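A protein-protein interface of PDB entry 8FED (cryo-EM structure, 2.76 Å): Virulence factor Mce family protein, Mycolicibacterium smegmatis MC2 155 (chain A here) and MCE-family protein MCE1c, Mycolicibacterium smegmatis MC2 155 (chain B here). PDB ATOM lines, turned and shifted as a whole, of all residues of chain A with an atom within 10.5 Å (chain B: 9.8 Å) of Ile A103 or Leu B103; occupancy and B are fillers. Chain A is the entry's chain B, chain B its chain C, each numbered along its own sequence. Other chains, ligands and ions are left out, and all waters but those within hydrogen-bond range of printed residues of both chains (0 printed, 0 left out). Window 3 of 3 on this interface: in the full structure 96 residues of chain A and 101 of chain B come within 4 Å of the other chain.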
ATOM      1  N   SER A  47      17.093  32.835  20.891  1.00  0.00           N
ATOM      2  CA  SER A  47      18.017  31.724  21.130  1.00  0.00           C
ATOM      3  C   SER A  47      18.949  32.002  22.314  1.00  0.00           C
ATOM      4  O   SER A  47      20.171  32.067  22.178  1.00  0.00           O
ATOM      5  CB  SER A  47      18.820  31.399  19.866  1.00  0.00           C
ATOM      6  OG  SER A  47      19.709  32.452  19.546  1.00  0.00           O
ATOM      7  N   GLY A  48      18.343  32.164  23.487  1.00  0.00           N
ATOM      8  CA  GLY A  48      19.122  32.275  24.703  1.00  0.00           C
ATOM      9  C   GLY A  48      19.859  33.579  24.888  1.00  0.00           C
ATOM     10  O   GLY A  48      20.835  33.622  25.639  1.00  0.00           O
ATOM     11  N   ARG A  50      20.494  36.998  26.565  1.00  0.00           N
ATOM     12  CA  ARG A  50      20.191  37.522  27.886  1.00  0.00           C
ATOM     13  C   ARG A  50      20.577  38.992  27.977  1.00  0.00           C
ATOM     14  O   ARG A  50      21.312  39.520  27.141  1.00  0.00           O
ATOM     15  CB  ARG A  50      20.918  36.733  28.981  1.00  0.00           C
ATOM     16  CG  ARG A  50      20.514  35.273  29.082  1.00  0.00           C
ATOM     17  CD  ARG A  50      21.202  34.569  30.249  1.00  0.00           C
ATOM     18  NE  ARG A  50      22.655  34.556  30.127  1.00  0.00           N
ATOM     19  CZ  ARG A  50      23.474  35.395  30.749  1.00  0.00           C
ATOM     20  NH1 ARG A  50      23.015  36.338  31.554  1.00  0.00           N
ATOM     21  NH2 ARG A  50      24.785  35.286  30.556  1.00  0.00           N
ATOM     22  N   GLN A  53      24.459  41.044  27.702  1.00  0.00           N
ATOM     23  CA  GLN A  53      25.360  40.507  26.695  1.00  0.00           C
ATOM     24  C   GLN A  53      25.679  41.572  25.654  1.00  0.00           C
ATOM     25  O   GLN A  53      24.860  42.444  25.357  1.00  0.00           O
ATOM     26  CB  GLN A  53      24.750  39.269  26.039  1.00  0.00           C
ATOM     27  CG  GLN A  53      24.797  38.039  26.933  1.00  0.00           C
ATOM     28  CD  GLN A  53      23.994  36.881  26.390  1.00  0.00           C
ATOM     29  OE1 GLN A  53      23.073  37.066  25.599  1.00  0.00           O
ATOM     30  NE2 GLN A  53      24.338  35.672  26.815  1.00  0.00           N
ATOM     31  N   ARG A  98      24.606  35.752  17.328  1.00  0.00           N
ATOM     32  CA  ARG A  98      25.708  34.852  17.033  1.00  0.00           C
ATOM     33  C   ARG A  98      26.195  34.173  18.306  1.00  0.00           C
ATOM     34  O   ARG A  98      26.090  34.725  19.406  1.00  0.00           O
ATOM     35  CB  ARG A  98      26.868  35.603  16.372  1.00  0.00           C
ATOM     36  CG  ARG A  98      26.535  36.240  15.030  1.00  0.00           C
ATOM     37  CD  ARG A  98      26.461  35.210  13.915  1.00  0.00           C
ATOM     38  NE  ARG A  98      25.131  34.629  13.779  1.00  0.00           N
ATOM     39  CZ  ARG A  98      24.298  34.894  12.782  1.00  0.00           C
ATOM     40  NH1 ARG A  98      24.634  35.712  11.800  1.00  0.00           N
ATOM     41  NH2 ARG A  98      23.098  34.318  12.770  1.00  0.00           N
ATOM     42  N   TYR A  99      26.726  32.964  18.137  1.00  0.00           N
ATOM     43  CA  TYR A  99      27.321  32.231  19.246  1.00  0.00           C
ATOM     44  C   TYR A  99      28.588  32.927  19.721  1.00  0.00           C
ATOM     45  O   TYR A  99      29.447  33.294  18.914  1.00  0.00           O
ATOM     46  CB  TYR A  99      27.661  30.799  18.827  1.00  0.00           C
ATOM     47  CG  TYR A  99      26.509  29.821  18.812  1.00  0.00           C
ATOM     48  CD1 TYR A  99      25.195  30.253  18.880  1.00  0.00           C
ATOM     49  CD2 TYR A  99      26.746  28.455  18.738  1.00  0.00           C
ATOM     50  CE1 TYR A  99      24.149  29.352  18.865  1.00  0.00           C
ATOM     51  CE2 TYR A  99      25.708  27.549  18.728  1.00  0.00           C
ATOM     52  CZ  TYR A  99      24.412  28.002  18.793  1.00  0.00           C
ATOM     53  OH  TYR A  99      23.374  27.102  18.782  1.00  0.00           O
ATOM     54  N   GLN A 100      28.708  33.105  21.037  1.00  0.00           N
ATOM     55  CA  GLN A 100      29.990  33.500  21.604  1.00  0.00           C
ATOM     56  C   GLN A 100      30.892  32.292  21.819  1.00  0.00           C
ATOM     57  O   GLN A 100      32.112  32.392  21.649  1.00  0.00           O
ATOM     58  CB  GLN A 100      29.782  34.254  22.918  1.00  0.00           C
ATOM     59  CG  GLN A 100      31.071  34.712  23.582  1.00  0.00           C
ATOM     60  CD  GLN A 100      30.846  35.290  24.961  1.00  0.00           C
ATOM     61  OE1 GLN A 100      29.730  35.671  25.314  1.00  0.00           O
ATOM     62  NE2 GLN A 100      31.907  35.354  25.756  1.00  0.00           N
ATOM     63  N   ASP A 101      30.309  31.150  22.167  1.00  0.00           N
ATOM     64  CA  ASP A 101      31.049  29.911  22.363  1.00  0.00           C
ATOM     65  C   ASP A 101      30.075  28.745  22.233  1.00  0.00           C
ATOM     66  O   ASP A 101      28.913  28.924  21.854  1.00  0.00           O
ATOM     67  CB  ASP A 101      31.757  29.907  23.722  1.00  0.00           C
ATOM     68  CG  ASP A 101      30.800  30.129  24.881  1.00  0.00           C
ATOM     69  OD1 ASP A 101      29.606  30.387  24.636  1.00  0.00           O
ATOM     70  OD2 ASP A 101      31.239  30.038  26.045  1.00  0.00           O
ATOM     71  N   LEU A 102      30.547  27.548  22.563  1.00  0.00           N
ATOM     72  CA  LEU A 102      29.729  26.345  22.536  1.00  0.00           C
ATOM     73  C   LEU A 102      29.094  26.036  23.886  1.00  0.00           C
ATOM     74  O   LEU A 102      28.470  24.981  24.036  1.00  0.00           O
ATOM     75  CB  LEU A 102      30.566  25.155  22.062  1.00  0.00           C
ATOM     76  CG  LEU A 102      31.086  25.251  20.625  1.00  0.00           C
ATOM     77  CD1 LEU A 102      32.034  24.108  20.309  1.00  0.00           C
ATOM     78  CD2 LEU A 102      29.930  25.275  19.640  1.00  0.00           C
ATOM     79  N   ILE A 103      29.242  26.925  24.867  1.00  0.00           N
ATOM     80  CA  ILE A 103      28.654  26.701  26.184  1.00  0.00           C
ATOM     81  C   ILE A 103      27.237  27.267  26.283  1.00  0.00           C
ATOM     82  O   ILE A 103      26.415  26.748  27.045  1.00  0.00           O
ATOM     83  CB  ILE A 103      29.578  27.296  27.263  1.00  0.00           C
ATOM     84  CG1 ILE A 103      30.976  26.692  27.146  1.00  0.00           C
ATOM     85  CG2 ILE A 103      29.044  27.030  28.659  1.00  0.00           C
ATOM     86  CD1 ILE A 103      30.988  25.181  27.209  1.00  0.00           C
ATOM     87  N   GLY A 104      26.917  28.300  25.509  1.00  0.00           N
ATOM     88  CA  GLY A 104      25.583  28.867  25.541  1.00  0.00           C
ATOM     89  C   GLY A 104      25.548  30.380  25.608  1.00  0.00           C
ATOM     90  O   GLY A 104      24.490  30.971  25.840  1.00  0.00           O
ATOM     91  N   ASN A 105      26.697  31.018  25.407  1.00  0.00           N
ATOM     92  CA  ASN A 105      26.790  32.471  25.428  1.00  0.00           C
ATOM     93  C   ASN A 105      26.539  33.026  24.032  1.00  0.00           C
ATOM     94  O   ASN A 105      27.072  32.509  23.046  1.00  0.00           O
ATOM     95  CB  ASN A 105      28.159  32.917  25.939  1.00  0.00           C
ATOM     96  CG  ASN A 105      28.492  32.335  27.295  1.00  0.00           C
ATOM     97  OD1 ASN A 105      27.605  32.071  28.106  1.00  0.00           O
ATOM     98  ND2 ASN A 105      29.778  32.128  27.550  1.00  0.00           N
ATOM     99  N   ARG A 106      25.728  34.076  23.953  1.00  0.00           N
ATOM    100  CA  ARG A 106      25.339  34.691  22.695  1.00  0.00           C
ATOM    101  C   ARG A 106      25.798  36.142  22.661  1.00  0.00           C
ATOM    102  O   ARG A 106      26.256  36.699  23.663  1.00  0.00           O
ATOM    103  CB  ARG A 106      23.820  34.624  22.497  1.00  0.00           C
ATOM    104  CG  ARG A 106      23.223  33.243  22.669  1.00  0.00           C
ATOM    105  CD  ARG A 106      23.547  32.344  21.497  1.00  0.00           C
ATOM    106  NE  ARG A 106      22.877  31.055  21.613  1.00  0.00           N
ATOM    107  CZ  ARG A 106      23.450  29.954  22.077  1.00  0.00           C
ATOM    108  NH1 ARG A 106      24.715  29.942  22.460  1.00  0.00           N
ATOM    109  NH2 ARG A 106      22.735  28.835  22.153  1.00  0.00           N
ATOM    110  N   LEU A 134      22.164  29.357  15.660  1.00  0.00           N
ATOM    111  CA  LEU A 134      22.282  28.056  15.006  1.00  0.00           C
ATOM    112  C   LEU A 134      21.065  27.170  15.256  1.00  0.00           C
ATOM    113  O   LEU A 134      20.576  26.513  14.329  1.00  0.00           O
ATOM    114  CB  LEU A 134      23.552  27.357  15.492  1.00  0.00           C
ATOM    115  CG  LEU A 134      24.312  26.320  14.656  1.00  0.00           C
ATOM    116  CD1 LEU A 134      25.596  25.960  15.379  1.00  0.00           C
ATOM    117  CD2 LEU A 134      23.507  25.060  14.377  1.00  0.00           C
ATOM    118  N   LEU A 136      20.972  24.364  17.458  1.00  0.00           N
ATOM    119  CA  LEU A 136      21.653  23.084  17.268  1.00  0.00           C
ATOM    120  C   LEU A 136      20.696  21.897  17.293  1.00  0.00           C
ATOM    121  O   LEU A 136      20.949  20.888  16.625  1.00  0.00           O
ATOM    122  CB  LEU A 136      22.729  22.915  18.342  1.00  0.00           C
ATOM    123  CG  LEU A 136      23.495  21.594  18.411  1.00  0.00           C
ATOM    124  CD1 LEU A 136      24.443  21.458  17.235  1.00  0.00           C
ATOM    125  CD2 LEU A 136      24.245  21.486  19.724  1.00  0.00           C
ATOM    126  N   VAL A 140      20.604  18.823  14.591  1.00  0.00           N
ATOM    127  CA  VAL A 140      20.725  17.408  14.932  1.00  0.00           C
ATOM    128  C   VAL A 140      19.506  16.632  14.447  1.00  0.00           C
ATOM    129  O   VAL A 140      19.634  15.532  13.897  1.00  0.00           O
ATOM    130  CB  VAL A 140      20.950  17.237  16.446  1.00  0.00           C
ATOM    131  CG1 VAL A 140      21.000  15.768  16.811  1.00  0.00           C
ATOM    132  CG2 VAL A 140      22.237  17.922  16.866  1.00  0.00           C
ATOM    133  N   GLY B  51      17.129  13.374  28.889  1.00  0.00           N
ATOM    134  CA  GLY B  51      18.210  13.993  29.626  1.00  0.00           C
ATOM    135  C   GLY B  51      17.839  15.256  30.362  1.00  0.00           C
ATOM    136  O   GLY B  51      18.727  15.917  30.913  1.00  0.00           O
ATOM    137  N   ASN B  53      16.744  17.719  33.234  1.00  0.00           N
ATOM    138  CA  ASN B  53      16.940  17.729  34.674  1.00  0.00           C
ATOM    139  C   ASN B  53      16.037  18.769  35.320  1.00  0.00           C
ATOM    140  O   ASN B  53      15.506  19.662  34.654  1.00  0.00           O
ATOM    141  CB  ASN B  53      18.403  18.019  35.041  1.00  0.00           C
ATOM    142  CG  ASN B  53      19.334  16.887  34.665  1.00  0.00           C
ATOM    143  OD1 ASN B  53      18.927  15.728  34.602  1.00  0.00           O
ATOM    144  ND2 ASN B  53      20.596  17.217  34.418  1.00  0.00           N
ATOM    145  N   ARG B  59      11.966  28.226  27.861  1.00  0.00           N
ATOM    146  CA  ARG B  59      12.115  29.468  27.121  1.00  0.00           C
ATOM    147  C   ARG B  59      11.005  29.608  26.093  1.00  0.00           C
ATOM    148  O   ARG B  59      10.639  28.636  25.427  1.00  0.00           O
ATOM    149  CB  ARG B  59      13.472  29.521  26.407  1.00  0.00           C
ATOM    150  CG  ARG B  59      14.591  28.809  27.142  1.00  0.00           C
ATOM    151  CD  ARG B  59      15.951  29.123  26.549  1.00  0.00           C
ATOM    152  NE  ARG B  59      16.048  28.747  25.144  1.00  0.00           N
ATOM    153  CZ  ARG B  59      17.182  28.714  24.458  1.00  0.00           C
ATOM    154  NH1 ARG B  59      18.340  29.008  25.024  1.00  0.00           N
ATOM    155  NH2 ARG B  59      17.153  28.374  23.173  1.00  0.00           N
ATOM    156  N   THR B  99      18.038  19.802  22.707  1.00  0.00           N
ATOM    157  CA  THR B  99      19.435  19.896  23.099  1.00  0.00           C
ATOM    158  C   THR B  99      19.927  21.323  22.898  1.00  0.00           C
ATOM    159  O   THR B  99      19.741  21.909  21.829  1.00  0.00           O
ATOM    160  CB  THR B  99      20.281  18.925  22.276  1.00  0.00           C
ATOM    161  OG1 THR B  99      19.679  17.625  22.301  1.00  0.00           O
ATOM    162  CG2 THR B  99      21.684  18.830  22.839  1.00  0.00           C
ATOM    163  N   ASP B 100      20.555  21.884  23.928  1.00  0.00           N
ATOM    164  CA  ASP B 100      21.021  23.262  23.855  1.00  0.00           C
ATOM    165  C   ASP B 100      22.443  23.355  23.310  1.00  0.00           C
ATOM    166  O   ASP B 100      22.703  24.122  22.379  1.00  0.00           O
ATOM    167  CB  ASP B 100      20.937  23.915  25.237  1.00  0.00           C
ATOM    168  CG  ASP B 100      21.173  25.411  25.194  1.00  0.00           C
ATOM    169  OD1 ASP B 100      21.149  25.992  24.088  1.00  0.00           O
ATOM    170  OD2 ASP B 100      21.385  26.009  26.270  1.00  0.00           O
ATOM    171  N   THR B 101      23.369  22.586  23.877  1.00  0.00           N
ATOM    172  CA  THR B 101      24.768  22.619  23.483  1.00  0.00           C
ATOM    173  C   THR B 101      25.250  21.208  23.172  1.00  0.00           C
ATOM    174  O   THR B 101      24.548  20.221  23.401  1.00  0.00           O
ATOM    175  CB  THR B 101      25.645  23.247  24.576  1.00  0.00           C
ATOM    176  OG1 THR B 101      25.484  22.520  25.799  1.00  0.00           O
ATOM    177  CG2 THR B 101      25.253  24.695  24.803  1.00  0.00           C
ATOM    178  N   ILE B 102      26.472  21.123  22.641  1.00  0.00           N
ATOM    179  CA  ILE B 102      27.040  19.832  22.273  1.00  0.00           C
ATOM    180  C   ILE B 102      27.404  19.000  23.496  1.00  0.00           C
ATOM    181  O   ILE B 102      27.576  17.782  23.380  1.00  0.00           O
ATOM    182  CB  ILE B 102      28.275  20.018  21.375  1.00  0.00           C
ATOM    183  CG1 ILE B 102      29.392  20.721  22.147  1.00  0.00           C
ATOM    184  CG2 ILE B 102      27.913  20.805  20.127  1.00  0.00           C
ATOM    185  CD1 ILE B 102      30.687  20.819  21.386  1.00  0.00           C
ATOM    186  N   LEU B 103      27.529  19.623  24.666  1.00  0.00           N
ATOM    187  CA  LEU B 103      27.907  18.910  25.878  1.00  0.00           C
ATOM    188  C   LEU B 103      26.729  18.233  26.564  1.00  0.00           C
ATOM    189  O   LEU B 103      26.932  17.560  27.579  1.00  0.00           O
ATOM    190  CB  LEU B 103      28.596  19.867  26.853  1.00  0.00           C
ATOM    191  CG  LEU B 103      29.924  20.446  26.365  1.00  0.00           C
ATOM    192  CD1 LEU B 103      30.487  21.422  27.381  1.00  0.00           C
ATOM    193  CD2 LEU B 103      30.919  19.336  26.078  1.00  0.00           C
ATOM    194  N   GLY B 104      25.516  18.393  26.046  1.00  0.00           N
ATOM    195  CA  GLY B 104      24.370  17.653  26.531  1.00  0.00           C
ATOM    196  C   GLY B 104      23.337  18.441  27.307  1.00  0.00           C
ATOM    197  O   GLY B 104      22.412  17.831  27.855  1.00  0.00           O
ATOM    198  N   ARG B 105      23.459  19.764  27.379  1.00  0.00           N
ATOM    199  CA  ARG B 105      22.471  20.562  28.090  1.00  0.00           C
ATOM    200  C   ARG B 105      21.139  20.549  27.351  1.00  0.00           C
ATOM    201  O   ARG B 105      21.092  20.632  26.121  1.00  0.00           O
ATOM    202  CB  ARG B 105      22.966  21.997  28.259  1.00  0.00           C
ATOM    203  CG  ARG B 105      24.192  22.130  29.148  1.00  0.00           C
ATOM    204  CD  ARG B 105      23.982  21.462  30.498  1.00  0.00           C
ATOM    205  NE  ARG B 105      22.774  21.935  31.165  1.00  0.00           N
ATOM    206  CZ  ARG B 105      22.726  22.990  31.966  1.00  0.00           C
ATOM    207  NH1 ARG B 105      23.802  23.717  32.219  1.00  0.00           N
ATOM    208  NH2 ARG B 105      21.568  23.325  32.526  1.00  0.00           N
ATOM    209  N   LYS B 106      20.052  20.448  28.109  1.00  0.00           N
ATOM    210  CA  LYS B 106      18.711  20.354  27.554  1.00  0.00           C
ATOM    211  C   LYS B 106      17.847  21.488  28.086  1.00  0.00           C
ATOM    212  O   LYS B 106      18.069  21.992  29.191  1.00  0.00           O
ATOM    213  CB  LYS B 106      18.059  19.009  27.897  1.00  0.00           C
ATOM    214  CG  LYS B 106      18.902  17.795  27.554  1.00  0.00           C
ATOM    215  CD  LYS B 106      19.051  17.627  26.055  1.00  0.00           C
ATOM    216  CE  LYS B 106      19.968  16.464  25.727  1.00  0.00           C
ATOM    217  NZ  LYS B 106      19.471  15.192  26.308  1.00  0.00           N
ATOM    218  N   ASN B 107      16.858  21.887  27.291  1.00  0.00           N
ATOM    219  CA  ASN B 107      15.914  22.905  27.732  1.00  0.00           C
ATOM    220  C   ASN B 107      14.610  22.733  26.967  1.00  0.00           C
ATOM    221  O   ASN B 107      14.571  22.103  25.910  1.00  0.00           O
ATOM    222  CB  ASN B 107      16.474  24.320  27.546  1.00  0.00           C
ATOM    223  CG  ASN B 107      16.656  24.694  26.090  1.00  0.00           C
ATOM    224  OD1 ASN B 107      17.711  24.460  25.504  1.00  0.00           O
ATOM    225  ND2 ASN B 107      15.630  25.297  25.502  1.00  0.00           N
ATOM    226  N   GLN B 134      18.497  12.522  19.955  1.00  0.00           N
ATOM    227  CA  GLN B 134      19.743  12.596  20.701  1.00  0.00           C
ATOM    228  C   GLN B 134      20.951  12.558  19.774  1.00  0.00           C
ATOM    229  O   GLN B 134      20.921  11.955  18.700  1.00  0.00           O
ATOM    230  CB  GLN B 134      19.825  11.447  21.703  1.00  0.00           C
ATOM    231  CG  GLN B 134      18.575  11.254  22.542  1.00  0.00           C
ATOM    232  CD  GLN B 134      18.398  12.317  23.606  1.00  0.00           C
ATOM    233  OE1 GLN B 134      19.275  13.152  23.825  1.00  0.00           O
ATOM    234  NE2 GLN B 134      17.256  12.289  24.275  1.00  0.00           N
ATOM    235  N   ILE B 135      22.024  13.228  20.201  1.00  0.00           N
ATOM    236  CA  ILE B 135      23.267  13.204  19.436  1.00  0.00           C
ATOM    237  C   ILE B 135      23.840  11.793  19.399  1.00  0.00           C
ATOM    238  O   ILE B 135      24.329  11.329  18.360  1.00  0.00           O
ATOM    239  CB  ILE B 135      24.273  14.214  20.018  1.00  0.00           C
ATOM    240  CG1 ILE B 135      23.694  15.628  19.973  1.00  0.00           C
ATOM    241  CG2 ILE B 135      25.579  14.162  19.254  1.00  0.00           C
ATOM    242  CD1 ILE B 135      24.673  16.708  20.381  1.00  0.00           C
ATOM    243  N   TYR B 136      23.784  11.083  20.530  1.00  0.00           N
ATOM    244  CA  TYR B 136      24.249   9.702  20.543  1.00  0.00           C
ATOM    245  C   TYR B 136      23.360   8.807  19.690  1.00  0.00           C
ATOM    246  O   TYR B 136      23.852   7.845  19.093  1.00  0.00           O
ATOM    247  CB  TYR B 136      24.352   9.178  21.980  1.00  0.00           C
ATOM    248  CG  TYR B 136      23.058   9.105  22.768  1.00  0.00           C
ATOM    249  CD1 TYR B 136      22.206   8.015  22.650  1.00  0.00           C
ATOM    250  CD2 TYR B 136      22.713  10.109  23.661  1.00  0.00           C
ATOM    251  CE1 TYR B 136      21.036   7.942  23.376  1.00  0.00           C
ATOM    252  CE2 TYR B 136      21.547  10.041  24.394  1.00  0.00           C
ATOM    253  CZ  TYR B 136      20.712   8.957  24.246  1.00  0.00           C
ATOM    254  OH  TYR B 136      19.547   8.882  24.972  1.00  0.00           O
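The guanidinium group of Arg A106 lies within salt-bridge range of the side-chain carboxylate of Asp B100, 3.8 Å away.
The side-chain amide nitrogen (ND2) of Asn B107 lies close to the guanidinium group (NE) of Arg B59. N of Asp B100 sits at hydrogen-bond distance from O of Arg B105, at 2.6 Å. The backbone carbonyl oxygen of Ser A47 lies within hydrogen-bond range of the guanidinium group of Arg A106, at 2.9 Å. The side-chain carboxylate (OD1) of Asp A101 lies close to the backbone NH (N) of Ile A103, at 3.5 Å.
Among the printed residues, pairs that only touch across the chains: Ile A103 with Thr B101, Leu A102 with Thr B101, Gly A48 with Arg B59, Leu A136 with Thr B101, Leu A136 with Ile B102, Leu A102 with Ile B102 and Ile A103 with Leu B103.
Ile A103 touches two residues of chain B. Of the printed residues of chain A, Leu B103 touches Ile A103. No residue of chain B comes within 4 Å of Gly A104. Ile B102 touches just these residues of chain A: Leu A102 and Leu A136. No residue of chain A comes within 4 Å of Gly B104. Of the printed residues of chain A, Asp B100 touches Arg A106. Printed residues of chain B within 4 Å of Arg A106: Asp B100. The nearest residue of chain B that does not touch Ile A103 is Asp B100 (5.1 Å).
Printed residues of chain A that touch a printed residue of chain B: Gly A48, Leu A102, Ile A103, Arg A106 and Leu A136. Hydrophobic or aromatic side chains of chain A within 4 Å of the printed part of chain B: Leu A102, Ile A103 and Leu A136. Among the printed residues, 8 pairs touch across the chains. Among the printed residues, Asp or Glu carboxylates within 4 Å of a Lys or Arg side-chain nitrogen of the other chain: Arg A106 with Asp B100.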
